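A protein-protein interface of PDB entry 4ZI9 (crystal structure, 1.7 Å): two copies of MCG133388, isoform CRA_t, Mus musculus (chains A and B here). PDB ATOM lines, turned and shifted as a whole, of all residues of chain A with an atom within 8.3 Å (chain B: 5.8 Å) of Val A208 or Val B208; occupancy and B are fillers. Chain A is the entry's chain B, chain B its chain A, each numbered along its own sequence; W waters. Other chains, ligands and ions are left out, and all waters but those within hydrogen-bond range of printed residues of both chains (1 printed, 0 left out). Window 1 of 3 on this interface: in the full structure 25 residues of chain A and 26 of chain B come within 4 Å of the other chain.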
ATOM      1  N   MET A 115       2.231 -23.993  -8.332  1.00  0.00           N
ATOM      2  CA  MET A 115       1.257 -23.639  -9.358  1.00  0.00           C
ATOM      3  C   MET A 115       0.144 -24.668  -9.438  1.00  0.00           C
ATOM      4  O   MET A 115       0.407 -25.851  -9.619  1.00  0.00           O
ATOM      5  CB  MET A 115       1.928 -23.530 -10.728  1.00  0.00           C
ATOM      6  CG  MET A 115       3.077 -22.533 -10.819  1.00  0.00           C
ATOM      7  SD  MET A 115       3.688 -22.532 -12.512  1.00  0.00           S
ATOM      8  CE  MET A 115       2.446 -21.547 -13.333  1.00  0.00           C
ATOM      9  N   SER A 116      -1.098 -24.206  -9.356  1.00  0.00           N
ATOM     10  CA  SER A 116      -2.251 -25.074  -9.504  1.00  0.00           C
ATOM     11  C   SER A 116      -2.233 -25.740 -10.876  1.00  0.00           C
ATOM     12  O   SER A 116      -1.858 -25.111 -11.869  1.00  0.00           O
ATOM     13  CB  SER A 116      -3.541 -24.262  -9.322  1.00  0.00           C
ATOM     14  OG  SER A 116      -4.679 -25.084  -9.513  1.00  0.00           O
ATOM     15  N   GLU A 117      -2.686 -26.984 -10.955  1.00  0.00           N
ATOM     16  CA  GLU A 117      -2.755 -27.645 -12.247  1.00  0.00           C
ATOM     17  C   GLU A 117      -3.771 -26.982 -13.163  1.00  0.00           C
ATOM     18  O   GLU A 117      -3.786 -27.262 -14.361  1.00  0.00           O
ATOM     19  CB  GLU A 117      -3.072 -29.132 -12.084  1.00  0.00           C
ATOM     20  CG  GLU A 117      -4.343 -29.460 -11.312  1.00  0.00           C
ATOM     21  CD  GLU A 117      -4.589 -30.948 -11.282  1.00  0.00           C
ATOM     22  OE1 GLU A 117      -5.160 -31.444 -10.289  1.00  0.00           O
ATOM     23  OE2 GLU A 117      -4.199 -31.641 -12.252  1.00  0.00           O
ATOM     24  N   ILE A 118      -4.612 -26.104 -12.611  1.00  0.00           N
ATOM     25  CA  ILE A 118      -5.604 -25.382 -13.403  1.00  0.00           C
ATOM     26  C   ILE A 118      -5.120 -23.989 -13.871  1.00  0.00           C
ATOM     27  O   ILE A 118      -5.865 -23.255 -14.533  1.00  0.00           O
ATOM     28  CB  ILE A 118      -6.944 -25.238 -12.588  1.00  0.00           C
ATOM     29  CG1 ILE A 118      -8.144 -25.057 -13.491  1.00  0.00           C
ATOM     30  CG2 ILE A 118      -6.894 -24.089 -11.626  1.00  0.00           C
ATOM     31  CD1 ILE A 118      -9.438 -24.923 -12.701  1.00  0.00           C
ATOM     32  N   THR A 119      -3.872 -23.642 -13.557  1.00  0.00           N
ATOM     33  CA  THR A 119      -3.264 -22.396 -14.035  1.00  0.00           C
ATOM     34  C   THR A 119      -3.491 -22.235 -15.538  1.00  0.00           C
ATOM     35  O   THR A 119      -3.275 -23.182 -16.305  1.00  0.00           O
ATOM     36  CB  THR A 119      -1.759 -22.368 -13.753  1.00  0.00           C
ATOM     37  OG1 THR A 119      -1.523 -22.527 -12.350  1.00  0.00           O
ATOM     38  CG2 THR A 119      -1.130 -21.051 -14.220  1.00  0.00           C
ATOM     39  N   ASP A 174      -0.771 -30.942 -15.186  1.00  0.00           N
ATOM     40  CA  ASP A 174      -1.640 -32.038 -14.759  1.00  0.00           C
ATOM     41  C   ASP A 174      -0.945 -32.794 -13.644  1.00  0.00           C
ATOM     42  O   ASP A 174      -0.086 -33.631 -13.901  1.00  0.00           O
ATOM     43  CB  ASP A 174      -1.962 -32.988 -15.922  1.00  0.00           C
ATOM     44  CG  ASP A 174      -2.828 -34.183 -15.491  1.00  0.00           C
ATOM     45  OD1 ASP A 174      -3.347 -34.193 -14.358  1.00  0.00           O
ATOM     46  OD2 ASP A 174      -3.016 -35.106 -16.305  1.00  0.00           O
ATOM     47  N   ARG A 175      -1.331 -32.505 -12.404  1.00  0.00           N
ATOM     48  CA  ARG A 175      -0.709 -33.174 -11.263  1.00  0.00           C
ATOM     49  C   ARG A 175      -0.837 -34.707 -11.323  1.00  0.00           C
ATOM     50  O   ARG A 175       0.004 -35.410 -10.773  1.00  0.00           O
ATOM     51  CB  ARG A 175      -1.302 -32.638  -9.954  1.00  0.00           C
ATOM     52  CG  ARG A 175      -0.410 -32.902  -8.732  1.00  0.00           C
ATOM     53  CD  ARG A 175      -1.279 -33.046  -7.486  1.00  0.00           C
ATOM     54  NE  ARG A 175      -2.197 -34.176  -7.635  1.00  0.00           N
ATOM     55  CZ  ARG A 175      -1.909 -35.420  -7.279  1.00  0.00           C
ATOM     56  NH1 ARG A 175      -0.728 -35.717  -6.739  1.00  0.00           N
ATOM     57  NH2 ARG A 175      -2.798 -36.377  -7.469  1.00  0.00           N
ATOM     58  N   GLU A 176      -1.890 -35.239 -11.954  1.00  0.00           N
ATOM     59  CA  GLU A 176      -2.037 -36.693 -12.082  1.00  0.00           C
ATOM     60  C   GLU A 176      -1.047 -37.313 -13.094  1.00  0.00           C
ATOM     61  O   GLU A 176      -0.871 -38.528 -13.146  1.00  0.00           O
ATOM     62  CB  GLU A 176      -3.477 -37.062 -12.464  1.00  0.00           C
ATOM     63  CG  GLU A 176      -4.445 -36.965 -11.293  1.00  0.00           C
ATOM     64  CD  GLU A 176      -4.736 -35.548 -10.836  1.00  0.00           C
ATOM     65  OE1 GLU A 176      -5.131 -34.657 -11.646  1.00  0.00           O
ATOM     66  OE2 GLU A 176      -4.527 -35.296  -9.631  1.00  0.00           O
ATOM     67  N   VAL A 205       3.215 -28.844  -8.457  1.00  0.00           N
ATOM     68  CA  VAL A 205       1.904 -28.718  -9.075  1.00  0.00           C
ATOM     69  C   VAL A 205       0.812 -28.988  -8.045  1.00  0.00           C
ATOM     70  O   VAL A 205       0.744 -30.066  -7.462  1.00  0.00           O
ATOM     71  CB  VAL A 205       1.753 -29.670 -10.272  1.00  0.00           C
ATOM     72  CG1 VAL A 205       0.338 -29.529 -10.927  1.00  0.00           C
ATOM     73  CG2 VAL A 205       2.891 -29.419 -11.275  1.00  0.00           C
ATOM     74  N   VAL A 206      -0.028 -27.989  -7.819  1.00  0.00           N
ATOM     75  CA  VAL A 206      -1.020 -28.071  -6.771  1.00  0.00           C
ATOM     76  C   VAL A 206      -2.301 -28.733  -7.272  1.00  0.00           C
ATOM     77  O   VAL A 206      -2.821 -28.400  -8.351  1.00  0.00           O
ATOM     78  CB  VAL A 206      -1.333 -26.686  -6.206  1.00  0.00           C
ATOM     79  CG1 VAL A 206      -2.339 -26.815  -5.085  1.00  0.00           C
ATOM     80  CG2 VAL A 206      -0.049 -26.053  -5.718  1.00  0.00           C
ATOM     81  N   ASP A 207      -2.819 -29.666  -6.481  1.00  0.00           N
ATOM     82  CA  ASP A 207      -3.955 -30.477  -6.903  1.00  0.00           C
ATOM     83  C   ASP A 207      -5.236 -29.669  -7.042  1.00  0.00           C
ATOM     84  O   ASP A 207      -5.484 -28.722  -6.282  1.00  0.00           O
ATOM     85  CB  ASP A 207      -4.187 -31.634  -5.921  1.00  0.00           C
ATOM     86  CG  ASP A 207      -5.220 -32.651  -6.425  1.00  0.00           C
ATOM     87  OD1 ASP A 207      -5.121 -33.124  -7.583  1.00  0.00           O
ATOM     88  OD2 ASP A 207      -6.153 -32.994  -5.661  1.00  0.00           O
ATOM     89  N   VAL A 208      -6.020 -30.031  -8.050  1.00  0.00           N
ATOM     90  CA  VAL A 208      -7.416 -29.608  -8.175  1.00  0.00           C
ATOM     91  C   VAL A 208      -8.262 -30.895  -8.180  1.00  0.00           C
ATOM     92  O   VAL A 208      -7.802 -31.951  -8.660  1.00  0.00           O
ATOM     93  CB  VAL A 208      -7.672 -28.785  -9.460  1.00  0.00           C
ATOM     94  CG1 VAL A 208      -9.163 -28.579  -9.704  1.00  0.00           C
ATOM     95  CG2 VAL A 208      -6.911 -27.432  -9.413  1.00  0.00           C
ATOM     96  N   ASN A 209      -9.483 -30.835  -7.629  1.00  0.00           N
ATOM     97  CA  ASN A 209     -10.334 -32.017  -7.713  1.00  0.00           C
ATOM     98  C   ASN A 209     -10.872 -32.120  -9.114  1.00  0.00           C
ATOM     99  O   ASN A 209     -11.963 -31.652  -9.390  1.00  0.00           O
ATOM    100  CB  ASN A 209     -11.494 -31.986  -6.712  1.00  0.00           C
ATOM    101  CG  ASN A 209     -12.202 -33.343  -6.620  1.00  0.00           C
ATOM    102  OD1 ASN A 209     -11.584 -34.387  -6.854  1.00  0.00           O
ATOM    103  ND2 ASN A 209     -13.496 -33.333  -6.290  1.00  0.00           N
ATOM    104  N   ASP A 210     -10.123 -32.726 -10.019  1.00  0.00           N
ATOM    105  CA  ASP A 210     -10.589 -32.721 -11.397  1.00  0.00           C
ATOM    106  C   ASP A 210     -10.796 -34.123 -11.931  1.00  0.00           C
ATOM    107  O   ASP A 210     -10.968 -34.329 -13.140  1.00  0.00           O
ATOM    108  CB  ASP A 210      -9.633 -31.905 -12.288  1.00  0.00           C
ATOM    109  CG  ASP A 210      -8.178 -32.399 -12.264  1.00  0.00           C
ATOM    110  OD1 ASP A 210      -7.723 -33.106 -11.329  1.00  0.00           O
ATOM    111  OD2 ASP A 210      -7.461 -32.000 -13.207  1.00  0.00           O
ATOM    112  N   ASN A 211     -10.827 -35.087 -11.020  1.00  0.00           N
ATOM    113  CA  ASN A 211     -11.199 -36.452 -11.371  1.00  0.00           C
ATOM    114  C   ASN A 211     -12.277 -36.987 -10.453  1.00  0.00           C
ATOM    115  O   ASN A 211     -12.120 -36.949  -9.213  1.00  0.00           O
ATOM    116  CB  ASN A 211      -9.999 -37.396 -11.285  1.00  0.00           C
ATOM    117  CG  ASN A 211      -8.919 -37.037 -12.254  1.00  0.00           C
ATOM    118  OD1 ASN A 211      -8.870 -37.572 -13.361  1.00  0.00           O
ATOM    119  ND2 ASN A 211      -8.048 -36.109 -11.858  1.00  0.00           N
ATOM    120  N   PRO A 212     -13.348 -37.523 -11.045  1.00  0.00           N
ATOM    121  CA  PRO A 212     -14.349 -38.267 -10.286  1.00  0.00           C
ATOM    122  C   PRO A 212     -13.810 -39.625  -9.901  1.00  0.00           C
ATOM    123  O   PRO A 212     -12.866 -40.117 -10.528  1.00  0.00           O
ATOM    124  CB  PRO A 212     -15.489 -38.409 -11.280  1.00  0.00           C
ATOM    125  CG  PRO A 212     -14.789 -38.523 -12.579  1.00  0.00           C
ATOM    126  CD  PRO A 212     -13.649 -37.523 -12.487  1.00  0.00           C
ATOM    127  N   ASP A 241      -9.702 -43.124  -7.162  1.00  0.00           N
ATOM    128  CA  ASP A 241      -9.735 -41.704  -7.488  1.00  0.00           C
ATOM    129  C   ASP A 241      -8.303 -41.172  -7.412  1.00  0.00           C
ATOM    130  O   ASP A 241      -7.668 -41.272  -6.363  1.00  0.00           O
ATOM    131  CB  ASP A 241     -10.647 -40.941  -6.525  1.00  0.00           C
ATOM    132  CG  ASP A 241     -10.886 -39.500  -6.957  1.00  0.00           C
ATOM    133  OD1 ASP A 241      -9.916 -38.820  -7.392  1.00  0.00           O
ATOM    134  OD2 ASP A 241     -12.048 -39.042  -6.847  1.00  0.00           O
ATOM    135  N   PRO A 242      -7.791 -40.630  -8.520  1.00  0.00           N
ATOM    136  CA  PRO A 242      -6.366 -40.283  -8.587  1.00  0.00           C
ATOM    137  C   PRO A 242      -5.991 -38.928  -7.994  1.00  0.00           C
ATOM    138  O   PRO A 242      -4.808 -38.614  -7.939  1.00  0.00           O
ATOM    139  CB  PRO A 242      -6.093 -40.271 -10.091  1.00  0.00           C
ATOM    140  CG  PRO A 242      -7.365 -39.892 -10.698  1.00  0.00           C
ATOM    141  CD  PRO A 242      -8.451 -40.477  -9.829  1.00  0.00           C
ATOM    142  N   ASP A 243      -6.963 -38.131  -7.570  1.00  0.00           N
ATOM    143  CA  ASP A 243      -6.654 -36.832  -6.993  1.00  0.00           C
ATOM    144  C   ASP A 243      -6.026 -37.034  -5.625  1.00  0.00           C
ATOM    145  O   ASP A 243      -6.015 -38.152  -5.107  1.00  0.00           O
ATOM    146  CB  ASP A 243      -7.913 -35.961  -6.899  1.00  0.00           C
ATOM    147  CG  ASP A 243      -8.480 -35.623  -8.248  1.00  0.00           C
ATOM    148  OD1 ASP A 243      -7.734 -35.189  -9.150  1.00  0.00           O
ATOM    149  OD2 ASP A 243      -9.677 -35.842  -8.448  1.00  0.00           O
ATOM    150  N   GLU A 244      -5.517 -35.945  -5.046  1.00  0.00           N
ATOM    151  CA  GLU A 244      -4.709 -36.000  -3.824  1.00  0.00           C
ATOM    152  C   GLU A 244      -5.531 -35.741  -2.554  1.00  0.00           C
ATOM    153  O   GLU A 244      -6.430 -34.899  -2.546  1.00  0.00           O
ATOM    154  CB  GLU A 244      -3.566 -34.974  -3.922  1.00  0.00           C
ATOM    155  CG  GLU A 244      -2.697 -34.867  -2.668  1.00  0.00           C
ATOM    156  CD  GLU A 244      -1.525 -33.900  -2.841  1.00  0.00           C
ATOM    157  OE1 GLU A 244      -1.614 -32.993  -3.694  1.00  0.00           O
ATOM    158  OE2 GLU A 244      -0.518 -34.045  -2.115  1.00  0.00           O
ATOM    159  N   ASN A 247      -9.531 -34.994  -2.009  1.00  0.00           N
ATOM    160  CA  ASN A 247     -10.017 -35.020  -3.391  1.00  0.00           C
ATOM    161  C   ASN A 247     -10.056 -36.434  -3.994  1.00  0.00           C
ATOM    162  O   ASN A 247     -10.798 -36.697  -4.970  1.00  0.00           O
ATOM    163  CB  ASN A 247      -9.153 -34.107  -4.264  1.00  0.00           C
ATOM    164  CG  ASN A 247      -9.168 -32.664  -3.802  1.00  0.00           C
ATOM    165  OD1 ASN A 247     -10.136 -32.196  -3.208  1.00  0.00           O
ATOM    166  ND2 ASN A 247      -8.073 -31.951  -4.059  1.00  0.00           N
ATOM    167  N   GLY A 248      -9.256 -37.336  -3.428  1.00  0.00           N
ATOM    168  CA  GLY A 248      -9.197 -38.713  -3.885  1.00  0.00           C
ATOM    169  C   GLY A 248      -9.726 -39.745  -2.895  1.00  0.00           C
ATOM    170  O   GLY A 248      -9.666 -40.950  -3.149  1.00  0.00           O
ATOM    171  N   ASP A 296     -16.080 -38.545  -3.864  1.00  0.00           N
ATOM    172  CA  ASP A 296     -14.811 -38.125  -3.276  1.00  0.00           C
ATOM    173  C   ASP A 296     -15.071 -37.039  -2.228  1.00  0.00           C
ATOM    174  O   ASP A 296     -16.213 -36.740  -1.900  1.00  0.00           O
ATOM    175  CB  ASP A 296     -13.808 -37.657  -4.350  1.00  0.00           C
ATOM    176  CG  ASP A 296     -14.246 -36.409  -5.101  1.00  0.00           C
ATOM    177  OD1 ASP A 296     -14.996 -35.555  -4.560  1.00  0.00           O
ATOM    178  OD2 ASP A 296     -13.817 -36.284  -6.272  1.00  0.00           O
ATOM    179  N   ALA A 298     -14.832 -33.899  -2.322  1.00  0.00           N
ATOM    180  CA  ALA A 298     -15.020 -32.531  -2.811  1.00  0.00           C
ATOM    181  C   ALA A 298     -16.015 -32.429  -3.972  1.00  0.00           C
ATOM    182  O   ALA A 298     -15.865 -31.582  -4.859  1.00  0.00           O
ATOM    183  CB  ALA A 298     -13.648 -31.914  -3.221  1.00  0.00           C
ATOM    184  N   GLY A 299     -17.043 -33.272  -3.945  1.00  0.00           N
ATOM    185  CA  GLY A 299     -18.196 -33.085  -4.805  1.00  0.00           C
ATOM    186  C   GLY A 299     -18.184 -33.728  -6.172  1.00  0.00           C
ATOM    187  O   GLY A 299     -18.964 -33.343  -7.042  1.00  0.00           O
ATOM    188  N   LEU A 300     -17.305 -34.698  -6.392  1.00  0.00           N
ATOM    189  CA  LEU A 300     -17.424 -35.474  -7.616  1.00  0.00           C
ATOM    190  C   LEU A 300     -17.827 -36.894  -7.248  1.00  0.00           C
ATOM    191  O   LEU A 300     -17.532 -37.388  -6.154  1.00  0.00           O
ATOM    192  CB  LEU A 300     -16.124 -35.460  -8.426  1.00  0.00           C
ATOM    193  CG  LEU A 300     -15.665 -34.114  -9.013  1.00  0.00           C
ATOM    194  CD1 LEU A 300     -14.348 -34.311  -9.774  1.00  0.00           C
ATOM    195  CD2 LEU A 300     -16.724 -33.495  -9.931  1.00  0.00           C
ATOM    196  N   SER B 116     -19.618 -30.535  -7.312  1.00  0.00           N
ATOM    197  CA  SER B 116     -18.523 -29.626  -7.599  1.00  0.00           C
ATOM    198  C   SER B 116     -18.877 -28.723  -8.763  1.00  0.00           C
ATOM    199  O   SER B 116     -19.546 -29.155  -9.700  1.00  0.00           O
ATOM    200  CB  SER B 116     -17.259 -30.420  -7.919  1.00  0.00           C
ATOM    201  OG  SER B 116     -16.334 -29.599  -8.608  1.00  0.00           O
ATOM    202  N   GLU B 117     -18.406 -27.476  -8.738  1.00  0.00           N
ATOM    203  CA  GLU B 117     -18.701 -26.608  -9.867  1.00  0.00           C
ATOM    204  C   GLU B 117     -18.014 -27.073 -11.145  1.00  0.00           C
ATOM    205  O   GLU B 117     -18.399 -26.642 -12.250  1.00  0.00           O
ATOM    206  CB  GLU B 117     -18.331 -25.154  -9.551  1.00  0.00           C
ATOM    207  CG  GLU B 117     -16.897 -24.922  -9.105  1.00  0.00           C
ATOM    208  CD  GLU B 117     -16.615 -23.461  -8.920  1.00  0.00           C
ATOM    209  OE1 GLU B 117     -15.808 -23.114  -8.037  1.00  0.00           O
ATOM    210  OE2 GLU B 117     -17.219 -22.654  -9.657  1.00  0.00           O
ATOM    211  N   ILE B 118     -17.054 -27.990 -11.019  1.00  0.00           N
ATOM    212  CA  ILE B 118     -16.366 -28.516 -12.199  1.00  0.00           C
ATOM    213  C   ILE B 118     -17.000 -29.825 -12.730  1.00  0.00           C
ATOM    214  O   ILE B 118     -16.475 -30.446 -13.663  1.00  0.00           O
ATOM    215  CB  ILE B 118     -14.843 -28.708 -11.895  1.00  0.00           C
ATOM    216  CG1 ILE B 118     -14.003 -28.617 -13.161  1.00  0.00           C
ATOM    217  CG2 ILE B 118     -14.562 -30.011 -11.189  1.00  0.00           C
ATOM    218  CD1 ILE B 118     -12.500 -28.782 -12.878  1.00  0.00           C
ATOM    219  N   ARG B 175     -20.015 -21.848  -8.850  1.00  0.00           N
ATOM    220  CA  ARG B 175     -20.306 -21.405  -7.492  1.00  0.00           C
ATOM    221  C   ARG B 175     -20.201 -19.890  -7.326  1.00  0.00           C
ATOM    222  O   ARG B 175     -20.912 -19.312  -6.506  1.00  0.00           O
ATOM    223  CB  ARG B 175     -19.366 -22.100  -6.511  1.00  0.00           C
ATOM    224  CG  ARG B 175     -19.821 -22.093  -5.058  1.00  0.00           C
ATOM    225  CD  ARG B 175     -18.618 -22.131  -4.145  1.00  0.00           C
ATOM    226  NE  ARG B 175     -17.806 -20.929  -4.346  1.00  0.00           N
ATOM    227  CZ  ARG B 175     -17.956 -19.797  -3.660  1.00  0.00           C
ATOM    228  NH1 ARG B 175     -18.853 -19.716  -2.686  1.00  0.00           N
ATOM    229  NH2 ARG B 175     -17.194 -18.751  -3.928  1.00  0.00           N
ATOM    230  N   GLU B 176     -19.324 -19.234  -8.088  1.00  0.00           N
ATOM    231  CA  GLU B 176     -19.201 -17.784  -7.976  1.00  0.00           C
ATOM    232  C   GLU B 176     -20.402 -17.040  -8.590  1.00  0.00           C
ATOM    233  O   GLU B 176     -20.569 -15.847  -8.366  1.00  0.00           O
ATOM    234  CB  GLU B 176     -17.894 -17.295  -8.615  1.00  0.00           C
ATOM    235  CG  GLU B 176     -16.661 -17.578  -7.783  1.00  0.00           C
ATOM    236  CD  GLU B 176     -16.280 -19.056  -7.720  1.00  0.00           C
ATOM    237  OE1 GLU B 176     -16.218 -19.738  -8.779  1.00  0.00           O
ATOM    238  OE2 GLU B 176     -15.982 -19.540  -6.604  1.00  0.00           O
ATOM    239  N   VAL B 206     -20.121 -27.140  -4.894  1.00  0.00           N
ATOM    240  CA  VAL B 206     -18.875 -27.215  -4.152  1.00  0.00           C
ATOM    241  C   VAL B 206     -17.773 -26.422  -4.874  1.00  0.00           C
ATOM    242  O   VAL B 206     -17.627 -26.479  -6.110  1.00  0.00           O
ATOM    243  CB  VAL B 206     -18.439 -28.671  -3.928  1.00  0.00           C
ATOM    244  CG1 VAL B 206     -17.191 -28.710  -3.100  1.00  0.00           C
ATOM    245  CG2 VAL B 206     -19.539 -29.414  -3.201  1.00  0.00           C
ATOM    246  N   ASP B 207     -17.036 -25.641  -4.103  1.00  0.00           N
ATOM    247  CA  ASP B 207     -16.053 -24.725  -4.679  1.00  0.00           C
ATOM    248  C   ASP B 207     -14.883 -25.460  -5.331  1.00  0.00           C
ATOM    249  O   ASP B 207     -14.453 -26.522  -4.852  1.00  0.00           O
ATOM    250  CB  ASP B 207     -15.525 -23.768  -3.599  1.00  0.00           C
ATOM    251  CG  ASP B 207     -14.638 -22.650  -4.168  1.00  0.00           C
ATOM    252  OD1 ASP B 207     -14.951 -22.070  -5.233  1.00  0.00           O
ATOM    253  OD2 ASP B 207     -13.605 -22.360  -3.553  1.00  0.00           O
ATOM    254  N   VAL B 208     -14.397 -24.901  -6.437  1.00  0.00           N
ATOM    255  CA  VAL B 208     -13.074 -25.258  -6.990  1.00  0.00           C
ATOM    256  C   VAL B 208     -12.226 -23.981  -7.010  1.00  0.00           C
ATOM    257  O   VAL B 208     -12.776 -22.888  -7.218  1.00  0.00           O
ATOM    258  CB  VAL B 208     -13.206 -25.847  -8.410  1.00  0.00           C
ATOM    259  CG1 VAL B 208     -11.834 -26.015  -9.068  1.00  0.00           C
ATOM    260  CG2 VAL B 208     -13.977 -27.192  -8.367  1.00  0.00           C
ATOM    261  N   ASN B 209     -10.911 -24.087  -6.797  1.00  0.00           N
ATOM    262  CA  ASN B 209     -10.088 -22.893  -6.915  1.00  0.00           C
ATOM    263  C   ASN B 209      -9.932 -22.571  -8.381  1.00  0.00           C
ATOM    264  O   ASN B 209      -8.949 -22.981  -8.996  1.00  0.00           O
ATOM    265  CB  ASN B 209      -8.717 -23.068  -6.279  1.00  0.00           C
ATOM    266  CG  ASN B 209      -7.985 -21.731  -6.134  1.00  0.00           C
ATOM    267  OD1 ASN B 209      -8.627 -20.669  -5.985  1.00  0.00           O
ATOM    268  ND2 ASN B 209      -6.650 -21.764  -6.198  1.00  0.00           N
ATOM    269  N   ASP B 210     -10.882 -21.847  -8.946  1.00  0.00           N
ATOM    270  CA  ASP B 210     -10.814 -21.584 -10.377  1.00  0.00           C
ATOM    271  C   ASP B 210     -10.733 -20.095 -10.707  1.00  0.00           C
ATOM    272  O   ASP B 210     -10.957 -19.686 -11.856  1.00  0.00           O
ATOM    273  CB  ASP B 210     -11.993 -22.257 -11.112  1.00  0.00           C
ATOM    274  CG  ASP B 210     -13.376 -21.842 -10.592  1.00  0.00           C
ATOM    275  OD1 ASP B 210     -13.526 -21.370  -9.443  1.00  0.00           O
ATOM    276  OD2 ASP B 210     -14.341 -22.011 -11.364  1.00  0.00           O
ATOM    277  N   ASN B 211     -10.414 -19.278  -9.707  1.00  0.00           N
ATOM    278  CA  ASN B 211     -10.143 -17.855  -9.940  1.00  0.00           C
ATOM    279  C   ASN B 211      -8.831 -17.482  -9.293  1.00  0.00           C
ATOM    280  O   ASN B 211      -8.615 -17.788  -8.117  1.00  0.00           O
ATOM    281  CB  ASN B 211     -11.228 -16.940  -9.369  1.00  0.00           C
ATOM    282  CG  ASN B 211     -12.576 -17.155 -10.013  1.00  0.00           C
ATOM    283  OD1 ASN B 211     -12.938 -16.462 -10.961  1.00  0.00           O
ATOM    284  ND2 ASN B 211     -13.324 -18.137  -9.507  1.00  0.00           N
ATOM    285  N   ASP B 243     -13.166 -16.962  -4.886  1.00  0.00           N
ATOM    286  CA  ASP B 243     -13.337 -18.342  -4.449  1.00  0.00           C
ATOM    287  C   ASP B 243     -13.582 -18.400  -2.938  1.00  0.00           C
ATOM    288  O   ASP B 243     -13.463 -17.384  -2.234  1.00  0.00           O
ATOM    289  CB  ASP B 243     -12.124 -19.195  -4.825  1.00  0.00           C
ATOM    290  CG  ASP B 243     -11.946 -19.311  -6.318  1.00  0.00           C
ATOM    291  OD1 ASP B 243     -12.933 -19.576  -7.042  1.00  0.00           O
ATOM    292  OD2 ASP B 243     -10.827 -19.082  -6.782  1.00  0.00           O
ATOM    293  N   ASN B 247      -9.310 -20.983  -0.763  1.00  0.00           N
ATOM    294  CA  ASN B 247      -9.205 -20.703  -2.195  1.00  0.00           C
ATOM    295  C   ASN B 247      -9.298 -19.212  -2.548  1.00  0.00           C
ATOM    296  O   ASN B 247      -8.814 -18.794  -3.609  1.00  0.00           O
ATOM    297  CB  ASN B 247     -10.280 -21.470  -2.964  1.00  0.00           C
ATOM    298  CG  ASN B 247     -10.155 -22.956  -2.797  1.00  0.00           C
ATOM    299  OD1 ASN B 247      -9.067 -23.466  -2.544  1.00  0.00           O
ATOM    300  ND2 ASN B 247     -11.269 -23.673  -2.952  1.00  0.00           N
HETATM  301  O   HOH W   1     -14.288 -30.309  -7.161  1.00  0.00           O
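The backbone NH (N) of Ser B116 is in hydrogen-bond range of the backbone carbonyl oxygen (O) of Gly A299, at 2.9 Å.
The side-chain carboxylate (OD1) of Asp A296 lies within hydrogen-bond range of the backbone NH (N) of Leu A300 (3.1 Å).
O of Val B206 sits at hydrogen-bond distance from N of Glu B117, 2.9 Å away.
The side-chain amide nitrogen (ND2) of Asn A209 lies within hydrogen-bond range of the backbone carbonyl oxygen (O) of Ala A298 (3.3 Å).
The backbone NH (N) of Gly A299 is in hydrogen-bond range of the side-chain carboxylate (OD1) of Asp A296 (3.1 Å).
OG of Ser B116 sits at hydrogen-bond distance from N of Ile B118, at 3.0 Å.
The side-chain carboxylate (OD1) of Asp A296 lies within hydrogen-bond range of the backbone NH (N) of Ala A298 (2.8 Å).
Among the printed residues, merely in contact across the chains: Ile A118 with Asn B209 (3.5 Å), Ala A298 with Ser B116 (3.6 Å), Asn A209 with Ile B118 (3.6 Å), Ala A298 with Val B206 (3.6 Å), Leu A300 with Ser B116 (3.7 Å) and Val A208 with Val B208 (3.8 Å).
Of the printed residues of chain A, Val B208 touches Val A208.
No residue of chain A comes within 4 Å of Asp B207.
Of the printed residues of chain B, Ile A118 touches Asn B209.
Printed residues of chain B within 4 Å of Gly A299: Ser B116.
Of the printed residues of chain A, Ser B116 touches Ala A298, Gly A299 and Leu A300.
Of the printed residues of chain B, Leu A300 touches Ser B116 (3.7 Å).
Printed residues of chain B within 4 Å of Ala A298: Ser B116 and Val B206.
The nearest residue of chain A that does not touch Val B208 is Ile A118 (4.5 Å).
The nearest printed residue of chain B that does not touch Asn A209 is Ser B116 (4.9 Å).
Of the 26 printed residues of chain A, 6 touch a printed residue of chain B.
Printed residues of chain A that touch a printed residue of chain B: Ile A118, Val A208, Asn A209, Ala A298, Gly A299 and Leu A300.
Of the 13 printed residues of chain B, 5 touch a printed residue of chain A.
Among the printed residues, 7 pairs touch across the chains.
Ile A118 touches Asn B209, and with the chains exchanged Asn A209 touches Ile B118.
Val A208 touches its own counterpart, Val B208.
Water W1 lies within hydrogen-bond range of OG of Ser B116 (2.6 Å), O of Ala A298 (3.1 Å) and ND2 of Asn A209 (3.2 Å).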
